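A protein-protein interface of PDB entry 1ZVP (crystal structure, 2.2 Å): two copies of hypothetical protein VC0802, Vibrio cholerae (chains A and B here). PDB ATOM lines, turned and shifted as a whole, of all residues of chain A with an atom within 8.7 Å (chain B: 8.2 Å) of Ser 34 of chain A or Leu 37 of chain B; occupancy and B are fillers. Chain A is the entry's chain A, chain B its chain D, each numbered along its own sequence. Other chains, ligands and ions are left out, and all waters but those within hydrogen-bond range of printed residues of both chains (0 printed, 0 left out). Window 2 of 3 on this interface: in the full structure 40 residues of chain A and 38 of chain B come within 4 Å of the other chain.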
ATOM      1  N   GLY A  31     -16.745  -8.185 -25.856  1.00  0.00           N
ATOM      2  CA  GLY A  31     -16.699  -9.313 -24.948  1.00  0.00           C
ATOM      3  C   GLY A  31     -18.060  -9.935 -24.783  1.00  0.00           C
ATOM      4  O   GLY A  31     -19.047  -9.461 -25.358  1.00  0.00           O
ATOM      5  N   ALA A  32     -18.102 -11.012 -24.007  1.00  0.00           N
ATOM      6  CA  ALA A  32     -19.355 -11.646 -23.646  1.00  0.00           C
ATOM      7  C   ALA A  32     -20.091 -10.765 -22.637  1.00  0.00           C
ATOM      8  O   ALA A  32     -19.473 -10.087 -21.809  1.00  0.00           O
ATOM      9  CB  ALA A  32     -19.096 -13.037 -23.067  1.00  0.00           C
ATOM     10  N   LEU A  33     -21.414 -10.766 -22.719  1.00  0.00           N
ATOM     11  CA  LEU A  33     -22.234 -10.062 -21.748  1.00  0.00           C
ATOM     12  C   LEU A  33     -21.876 -10.491 -20.316  1.00  0.00           C
ATOM     13  O   LEU A  33     -21.888  -9.668 -19.406  1.00  0.00           O
ATOM     14  CB  LEU A  33     -23.721 -10.279 -22.059  1.00  0.00           C
ATOM     15  CG  LEU A  33     -24.799  -9.744 -21.119  1.00  0.00           C
ATOM     16  CD1 LEU A  33     -24.648  -8.246 -20.875  1.00  0.00           C
ATOM     17  CD2 LEU A  33     -26.172 -10.068 -21.681  1.00  0.00           C
ATOM     18  N   SER A  34     -21.528 -11.763 -20.127  1.00  0.00           N
ATOM     19  CA  SER A  34     -21.170 -12.297 -18.804  1.00  0.00           C
ATOM     20  C   SER A  34     -19.990 -11.578 -18.132  1.00  0.00           C
ATOM     21  O   SER A  34     -19.931 -11.499 -16.905  1.00  0.00           O
ATOM     22  CB  SER A  34     -20.902 -13.806 -18.879  1.00  0.00           C
ATOM     23  OG  SER A  34     -19.891 -14.117 -19.827  1.00  0.00           O
ATOM     24  N   ASP A  35     -19.070 -11.044 -18.937  1.00  0.00           N
ATOM     25  CA  ASP A  35     -17.881 -10.330 -18.436  1.00  0.00           C
ATOM     26  C   ASP A  35     -18.170  -8.978 -17.796  1.00  0.00           C
ATOM     27  O   ASP A  35     -17.302  -8.405 -17.129  1.00  0.00           O
ATOM     28  CB  ASP A  35     -16.884 -10.110 -19.572  1.00  0.00           C
ATOM     29  CG  ASP A  35     -16.221 -11.388 -20.016  1.00  0.00           C
ATOM     30  OD1 ASP A  35     -15.999 -12.262 -19.148  1.00  0.00           O
ATOM     31  OD2 ASP A  35     -15.925 -11.512 -21.229  1.00  0.00           O
ATOM     32  N   TYR A  36     -19.381  -8.469 -18.016  1.00  0.00           N
ATOM     33  CA  TYR A  36     -19.735  -7.113 -17.635  1.00  0.00           C
ATOM     34  C   TYR A  36     -20.925  -7.086 -16.688  1.00  0.00           C
ATOM     35  O   TYR A  36     -21.524  -6.041 -16.465  1.00  0.00           O
ATOM     36  CB  TYR A  36     -19.996  -6.274 -18.893  1.00  0.00           C
ATOM     37  CG  TYR A  36     -18.776  -6.144 -19.772  1.00  0.00           C
ATOM     38  CD1 TYR A  36     -17.767  -5.232 -19.461  1.00  0.00           C
ATOM     39  CD2 TYR A  36     -18.615  -6.949 -20.898  1.00  0.00           C
ATOM     40  CE1 TYR A  36     -16.626  -5.116 -20.257  1.00  0.00           C
ATOM     41  CE2 TYR A  36     -17.473  -6.845 -21.701  1.00  0.00           C
ATOM     42  CZ  TYR A  36     -16.484  -5.928 -21.373  1.00  0.00           C
ATOM     43  OH  TYR A  36     -15.362  -5.808 -22.162  1.00  0.00           O
ATOM     44  N   LEU A  37     -21.252  -8.238 -16.117  1.00  0.00           N
ATOM     45  CA  LEU A  37     -22.367  -8.342 -15.183  1.00  0.00           C
ATOM     46  C   LEU A  37     -22.149  -7.567 -13.871  1.00  0.00           C
ATOM     47  O   LEU A  37     -23.097  -6.979 -13.328  1.00  0.00           O
ATOM     48  CB  LEU A  37     -22.697  -9.816 -14.909  1.00  0.00           C
ATOM     49  CG  LEU A  37     -23.864 -10.459 -15.674  1.00  0.00           C
ATOM     50  CD1 LEU A  37     -25.189 -10.215 -14.973  1.00  0.00           C
ATOM     51  CD2 LEU A  37     -23.957  -9.981 -17.110  1.00  0.00           C
ATOM     52  N   SER A  38     -20.907  -7.546 -13.381  1.00  0.00           N
ATOM     53  CA  SER A  38     -20.582  -6.871 -12.118  1.00  0.00           C
ATOM     54  C   SER A  38     -20.718  -5.357 -12.222  1.00  0.00           C
ATOM     55  O   SER A  38     -20.834  -4.675 -11.199  1.00  0.00           O
ATOM     56  CB  SER A  38     -19.173  -7.220 -11.650  1.00  0.00           C
ATOM     57  OG  SER A  38     -18.214  -6.437 -12.336  1.00  0.00           O
ATOM     58  N   LEU A  39     -20.696  -4.844 -13.454  1.00  0.00           N
ATOM     59  CA  LEU A  39     -20.917  -3.417 -13.724  1.00  0.00           C
ATOM     60  C   LEU A  39     -22.375  -2.982 -13.526  1.00  0.00           C
ATOM     61  O   LEU A  39     -22.659  -1.785 -13.414  1.00  0.00           O
ATOM     62  CB  LEU A  39     -20.422  -3.043 -15.127  1.00  0.00           C
ATOM     63  CG  LEU A  39     -18.904  -3.071 -15.337  1.00  0.00           C
ATOM     64  CD1 LEU A  39     -18.540  -2.749 -16.765  1.00  0.00           C
ATOM     65  CD2 LEU A  39     -18.201  -2.112 -14.394  1.00  0.00           C
ATOM     66  N   THR A  44     -28.594  -2.885 -22.148  1.00  0.00           N
ATOM     67  CA  THR A  44     -27.675  -3.720 -22.899  1.00  0.00           C
ATOM     68  C   THR A  44     -28.210  -3.823 -24.336  1.00  0.00           C
ATOM     69  O   THR A  44     -29.416  -3.967 -24.540  1.00  0.00           O
ATOM     70  CB  THR A  44     -27.593  -5.104 -22.192  1.00  0.00           C
ATOM     71  OG1 THR A  44     -26.512  -5.089 -21.259  1.00  0.00           O
ATOM     72  CG2 THR A  44     -27.399  -6.230 -23.136  1.00  0.00           C
ATOM     73  N   ARG A  46     -26.692  -5.821 -27.990  1.00  0.00           N
ATOM     74  CA  ARG A  46     -25.651  -6.462 -28.779  1.00  0.00           C
ATOM     75  C   ARG A  46     -25.692  -5.946 -30.237  1.00  0.00           C
ATOM     76  O   ARG A  46     -26.555  -6.345 -31.030  1.00  0.00           O
ATOM     77  CB  ARG A  46     -25.792  -7.990 -28.677  1.00  0.00           C
ATOM     78  CG  ARG A  46     -24.823  -8.799 -29.530  1.00  0.00           C
ATOM     79  CD  ARG A  46     -23.358  -8.521 -29.187  1.00  0.00           C
ATOM     80  NE  ARG A  46     -22.974  -9.061 -27.879  1.00  0.00           N
ATOM     81  CZ  ARG A  46     -21.741  -9.035 -27.371  1.00  0.00           C
ATOM     82  NH1 ARG A  46     -20.738  -8.488 -28.052  1.00  0.00           N
ATOM     83  NH2 ARG A  46     -21.509  -9.560 -26.171  1.00  0.00           N
ATOM     84  N   LEU A  51     -20.891  -4.987 -27.829  1.00  0.00           N
ATOM     85  CA  LEU A  51     -21.903  -4.812 -26.788  1.00  0.00           C
ATOM     86  C   LEU A  51     -22.049  -3.357 -26.362  1.00  0.00           C
ATOM     87  O   LEU A  51     -21.074  -2.739 -25.915  1.00  0.00           O
ATOM     88  CB  LEU A  51     -21.510  -5.617 -25.547  1.00  0.00           C
ATOM     89  CG  LEU A  51     -22.480  -6.482 -24.742  1.00  0.00           C
ATOM     90  CD1 LEU A  51     -21.950  -6.577 -23.320  1.00  0.00           C
ATOM     91  CD2 LEU A  51     -23.907  -6.009 -24.758  1.00  0.00           C
ATOM     92  N   LEU A  53     -23.244  -1.027 -23.543  1.00  0.00           N
ATOM     93  CA  LEU A  53     -23.613  -0.948 -22.130  1.00  0.00           C
ATOM     94  C   LEU A  53     -24.096   0.449 -21.806  1.00  0.00           C
ATOM     95  O   LEU A  53     -23.437   1.427 -22.150  1.00  0.00           O
ATOM     96  CB  LEU A  53     -22.423  -1.293 -21.231  1.00  0.00           C
ATOM     97  CG  LEU A  53     -21.782  -2.661 -21.428  1.00  0.00           C
ATOM     98  CD1 LEU A  53     -20.557  -2.765 -20.542  1.00  0.00           C
ATOM     99  CD2 LEU A  53     -22.772  -3.779 -21.121  1.00  0.00           C
ATOM    100  N   ALA B  32     -32.215 -11.763 -11.525  1.00  0.00           N
ATOM    101  CA  ALA B  32     -30.949 -11.274 -12.049  1.00  0.00           C
ATOM    102  C   ALA B  32     -30.760 -11.591 -13.524  1.00  0.00           C
ATOM    103  O   ALA B  32     -31.231 -12.618 -14.008  1.00  0.00           O
ATOM    104  CB  ALA B  32     -29.788 -11.829 -11.224  1.00  0.00           C
ATOM    105  N   LEU B  33     -30.072 -10.689 -14.225  1.00  0.00           N
ATOM    106  CA  LEU B  33     -29.668 -10.895 -15.616  1.00  0.00           C
ATOM    107  C   LEU B  33     -28.822 -12.168 -15.755  1.00  0.00           C
ATOM    108  O   LEU B  33     -28.956 -12.905 -16.742  1.00  0.00           O
ATOM    109  CB  LEU B  33     -28.866  -9.685 -16.120  1.00  0.00           C
ATOM    110  CG  LEU B  33     -28.831  -9.201 -17.583  1.00  0.00           C
ATOM    111  CD1 LEU B  33     -27.419  -8.729 -17.910  1.00  0.00           C
ATOM    112  CD2 LEU B  33     -29.303 -10.213 -18.631  1.00  0.00           C
ATOM    113  N   SER B  34     -27.967 -12.421 -14.756  1.00  0.00           N
ATOM    114  CA  SER B  34     -27.094 -13.608 -14.713  1.00  0.00           C
ATOM    115  C   SER B  34     -27.839 -14.941 -14.852  1.00  0.00           C
ATOM    116  O   SER B  34     -27.286 -15.900 -15.387  1.00  0.00           O
ATOM    117  CB  SER B  34     -26.222 -13.600 -13.446  1.00  0.00           C
ATOM    118  OG  SER B  34     -26.922 -13.064 -12.330  1.00  0.00           O
ATOM    119  N   ASP B  35     -29.089 -14.983 -14.386  1.00  0.00           N
ATOM    120  CA  ASP B  35     -29.985 -16.137 -14.554  1.00  0.00           C
ATOM    121  C   ASP B  35     -30.365 -16.403 -16.020  1.00  0.00           C
ATOM    122  O   ASP B  35     -30.725 -17.530 -16.378  1.00  0.00           O
ATOM    123  CB  ASP B  35     -31.283 -15.938 -13.751  1.00  0.00           C
ATOM    124  CG  ASP B  35     -31.047 -15.770 -12.245  1.00  0.00           C
ATOM    125  OD1 ASP B  35     -30.304 -16.587 -11.654  1.00  0.00           O
ATOM    126  OD2 ASP B  35     -31.633 -14.832 -11.650  1.00  0.00           O
ATOM    127  N   TYR B  36     -30.291 -15.369 -16.860  1.00  0.00           N
ATOM    128  CA  TYR B  36     -30.849 -15.427 -18.215  1.00  0.00           C
ATOM    129  C   TYR B  36     -29.820 -15.328 -19.342  1.00  0.00           C
ATOM    130  O   TYR B  36     -30.179 -15.345 -20.518  1.00  0.00           O
ATOM    131  CB  TYR B  36     -31.939 -14.360 -18.381  1.00  0.00           C
ATOM    132  CG  TYR B  36     -33.129 -14.563 -17.468  1.00  0.00           C
ATOM    133  CD1 TYR B  36     -34.202 -15.368 -17.856  1.00  0.00           C
ATOM    134  CD2 TYR B  36     -33.179 -13.957 -16.214  1.00  0.00           C
ATOM    135  CE1 TYR B  36     -35.300 -15.564 -17.016  1.00  0.00           C
ATOM    136  CE2 TYR B  36     -34.271 -14.143 -15.362  1.00  0.00           C
ATOM    137  CZ  TYR B  36     -35.328 -14.950 -15.768  1.00  0.00           C
ATOM    138  OH  TYR B  36     -36.412 -15.135 -14.934  1.00  0.00           O
ATOM    139  N   LEU B  37     -28.545 -15.242 -18.971  1.00  0.00           N
ATOM    140  CA  LEU B  37     -27.435 -15.148 -19.925  1.00  0.00           C
ATOM    141  C   LEU B  37     -27.463 -16.203 -21.033  1.00  0.00           C
ATOM    142  O   LEU B  37     -27.153 -15.896 -22.185  1.00  0.00           O
ATOM    143  CB  LEU B  37     -26.095 -15.210 -19.177  1.00  0.00           C
ATOM    144  CG  LEU B  37     -25.234 -13.957 -18.952  1.00  0.00           C
ATOM    145  CD1 LEU B  37     -26.033 -12.677 -18.923  1.00  0.00           C
ATOM    146  CD2 LEU B  37     -24.418 -14.108 -17.671  1.00  0.00           C
ATOM    147  N   SER B  38     -27.831 -17.435 -20.676  1.00  0.00           N
ATOM    148  CA  SER B  38     -27.856 -18.562 -21.619  1.00  0.00           C
ATOM    149  C   SER B  38     -28.894 -18.390 -22.726  1.00  0.00           C
ATOM    150  O   SER B  38     -28.821 -19.062 -23.756  1.00  0.00           O
ATOM    151  CB  SER B  38     -28.095 -19.884 -20.884  1.00  0.00           C
ATOM    152  OG  SER B  38     -29.297 -19.826 -20.136  1.00  0.00           O
ATOM    153  N   LEU B  39     -29.855 -17.492 -22.510  1.00  0.00           N
ATOM    154  CA  LEU B  39     -30.850 -17.161 -23.527  1.00  0.00           C
ATOM    155  C   LEU B  39     -30.290 -16.235 -24.617  1.00  0.00           C
ATOM    156  O   LEU B  39     -30.885 -16.105 -25.691  1.00  0.00           O
ATOM    157  CB  LEU B  39     -32.092 -16.534 -22.884  1.00  0.00           C
ATOM    158  CG  LEU B  39     -32.915 -17.383 -21.914  1.00  0.00           C
ATOM    159  CD1 LEU B  39     -34.077 -16.577 -21.363  1.00  0.00           C
ATOM    160  CD2 LEU B  39     -33.412 -18.645 -22.590  1.00  0.00           C
ATOM    161  N   GLU B  40     -29.145 -15.612 -24.324  1.00  0.00           N
ATOM    162  CA  GLU B  40     -28.434 -14.705 -25.238  1.00  0.00           C
ATOM    163  C   GLU B  40     -29.309 -13.569 -25.769  1.00  0.00           C
ATOM    164  O   GLU B  40     -29.470 -13.431 -26.986  1.00  0.00           O
ATOM    165  CB  GLU B  40     -27.809 -15.474 -26.401  1.00  0.00           C
ATOM    166  CG  GLU B  40     -26.624 -16.341 -26.016  1.00  0.00           C
ATOM    167  CD  GLU B  40     -26.448 -17.532 -26.953  1.00  0.00           C
ATOM    168  OE1 GLU B  40     -25.884 -18.556 -26.504  1.00  0.00           O
ATOM    169  OE2 GLU B  40     -26.880 -17.456 -28.130  1.00  0.00           O
ATOM    170  N   PRO B  41     -29.877 -12.752 -24.860  1.00  0.00           N
ATOM    171  CA  PRO B  41     -30.760 -11.676 -25.287  1.00  0.00           C
ATOM    172  C   PRO B  41     -30.016 -10.615 -26.100  1.00  0.00           C
ATOM    173  O   PRO B  41     -28.885 -10.265 -25.762  1.00  0.00           O
ATOM    174  CB  PRO B  41     -31.261 -11.092 -23.963  1.00  0.00           C
ATOM    175  CG  PRO B  41     -30.232 -11.461 -22.969  1.00  0.00           C
ATOM    176  CD  PRO B  41     -29.724 -12.785 -23.393  1.00  0.00           C
ATOM    177  N   THR B  44     -31.384  -5.765 -23.271  1.00  0.00           N
ATOM    178  CA  THR B  44     -31.705  -5.893 -21.851  1.00  0.00           C
ATOM    179  C   THR B  44     -32.109  -4.530 -21.305  1.00  0.00           C
ATOM    180  O   THR B  44     -31.498  -3.524 -21.647  1.00  0.00           O
ATOM    181  CB  THR B  44     -30.473  -6.419 -21.099  1.00  0.00           C
ATOM    182  OG1 THR B  44     -30.499  -7.843 -21.115  1.00  0.00           O
ATOM    183  CG2 THR B  44     -30.423  -5.936 -19.676  1.00  0.00           C
ATOM    184  N   LEU B  51     -36.815  -7.118 -15.150  1.00  0.00           N
ATOM    185  CA  LEU B  51     -35.864  -7.142 -16.261  1.00  0.00           C
ATOM    186  C   LEU B  51     -36.569  -7.366 -17.581  1.00  0.00           C
ATOM    187  O   LEU B  51     -37.258  -8.370 -17.753  1.00  0.00           O
ATOM    188  CB  LEU B  51     -34.835  -8.249 -16.035  1.00  0.00           C
ATOM    189  CG  LEU B  51     -33.632  -8.397 -16.955  1.00  0.00           C
ATOM    190  CD1 LEU B  51     -32.614  -7.287 -16.737  1.00  0.00           C
ATOM    191  CD2 LEU B  51     -33.000  -9.741 -16.684  1.00  0.00           C
ATOM    192  N   LEU B  53     -36.212  -8.436 -21.345  1.00  0.00           N
ATOM    193  CA  LEU B  53     -35.330  -9.147 -22.260  1.00  0.00           C
ATOM    194  C   LEU B  53     -35.910  -9.060 -23.652  1.00  0.00           C
ATOM    195  O   LEU B  53     -37.110  -9.231 -23.825  1.00  0.00           O
ATOM    196  CB  LEU B  53     -35.169 -10.623 -21.871  1.00  0.00           C
ATOM    197  CG  LEU B  53     -34.631 -11.013 -20.486  1.00  0.00           C
ATOM    198  CD1 LEU B  53     -34.767 -12.530 -20.260  1.00  0.00           C
ATOM    199  CD2 LEU B  53     -33.184 -10.551 -20.272  1.00  0.00           C
ATOM    200  N   LEU B  55     -35.476 -11.048 -27.084  1.00  0.00           N
ATOM    201  CA  LEU B  55     -34.981 -12.377 -27.384  1.00  0.00           C
ATOM    202  C   LEU B  55     -35.512 -12.837 -28.714  1.00  0.00           C
ATOM    203  O   LEU B  55     -36.605 -12.441 -29.109  1.00  0.00           O
ATOM    204  CB  LEU B  55     -35.504 -13.365 -26.334  1.00  0.00           C
ATOM    205  CG  LEU B  55     -35.073 -13.238 -24.878  1.00  0.00           C
ATOM    206  CD1 LEU B  55     -36.158 -13.739 -23.965  1.00  0.00           C
ATOM    207  CD2 LEU B  55     -33.806 -14.026 -24.672  1.00  0.00           C
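The backbone carbonyl oxygen of Thr 44 of chain A sits at hydrogen-bond distance from the backbone NH of Thr 44 of chain B, 3.0 Å away.
Among the printed residues, pairs that only touch across the chains: Leu 33 of chain A with Leu 37 of chain B, Ser 34 of chain A with Leu 37 of chain B, Leu 37 of chain A with Leu 33 of chain B, Leu 37 of chain A with Ser 34 of chain B and Leu 37 of chain A with Leu 37 of chain B.
Ser 34 of chain A touches just one residue of chain B: Leu 37 (3.7 Å).
Of the printed residues of chain A, Leu 37 of chain B touches Leu 33, Ser 34 and Leu 37.
Ser 38 of chain B touches none of the printed residues of chain A.
Of the printed residues of chain A, Thr 44 of chain B touches Thr 44.
Printed residues of chain B within 4 Å of Leu 37 of chain A: Leu 33, Ser 34 and Leu 37.
Of the printed residues of chain A, Leu 33 of chain B touches Leu 37.
Printed residues of chain B within 4 Å of Leu 33 of chain A: Leu 37 (3.8 Å).
Of the printed residues of chain B, Thr 44 of chain A touches Thr 44.
Leu 53 of chain B touches none of the printed residues of chain A.
The nearest printed residue of chain B that does not touch Leu 37 of chain A is Ala 32 of chain B (5.9 Å).
Hydrophobic or aromatic side chains of chain A within 4 Å of the printed part of chain B: Leu 33 and Leu 37.
Hydrophobic or aromatic side chains of chain B within 4 Å of the printed part of chain A: Leu 33 and Leu 37.
Among the printed residues, 6 pairs touch across the chains.
Among the printed residues, no Asp or Glu carboxylate lies within 4 Å of a Lys or Arg side-chain nitrogen of the other chain.
Leu 33 of chain A touches Leu 37 of chain B, and with the chains exchanged Leu 37 of chain A touches Leu 33 of chain B.
Ser 34 of chain A touches Leu 37 of chain B, and with the chains exchanged Leu 37 of chain A touches Ser 34 of chain B.
Leu 37 of chain B touches its own counterpart, Leu 37 of chain A.
Thr 44 of chain A touches its own counterpart, Thr 44 of chain B.
11 positions are printed for both chains.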
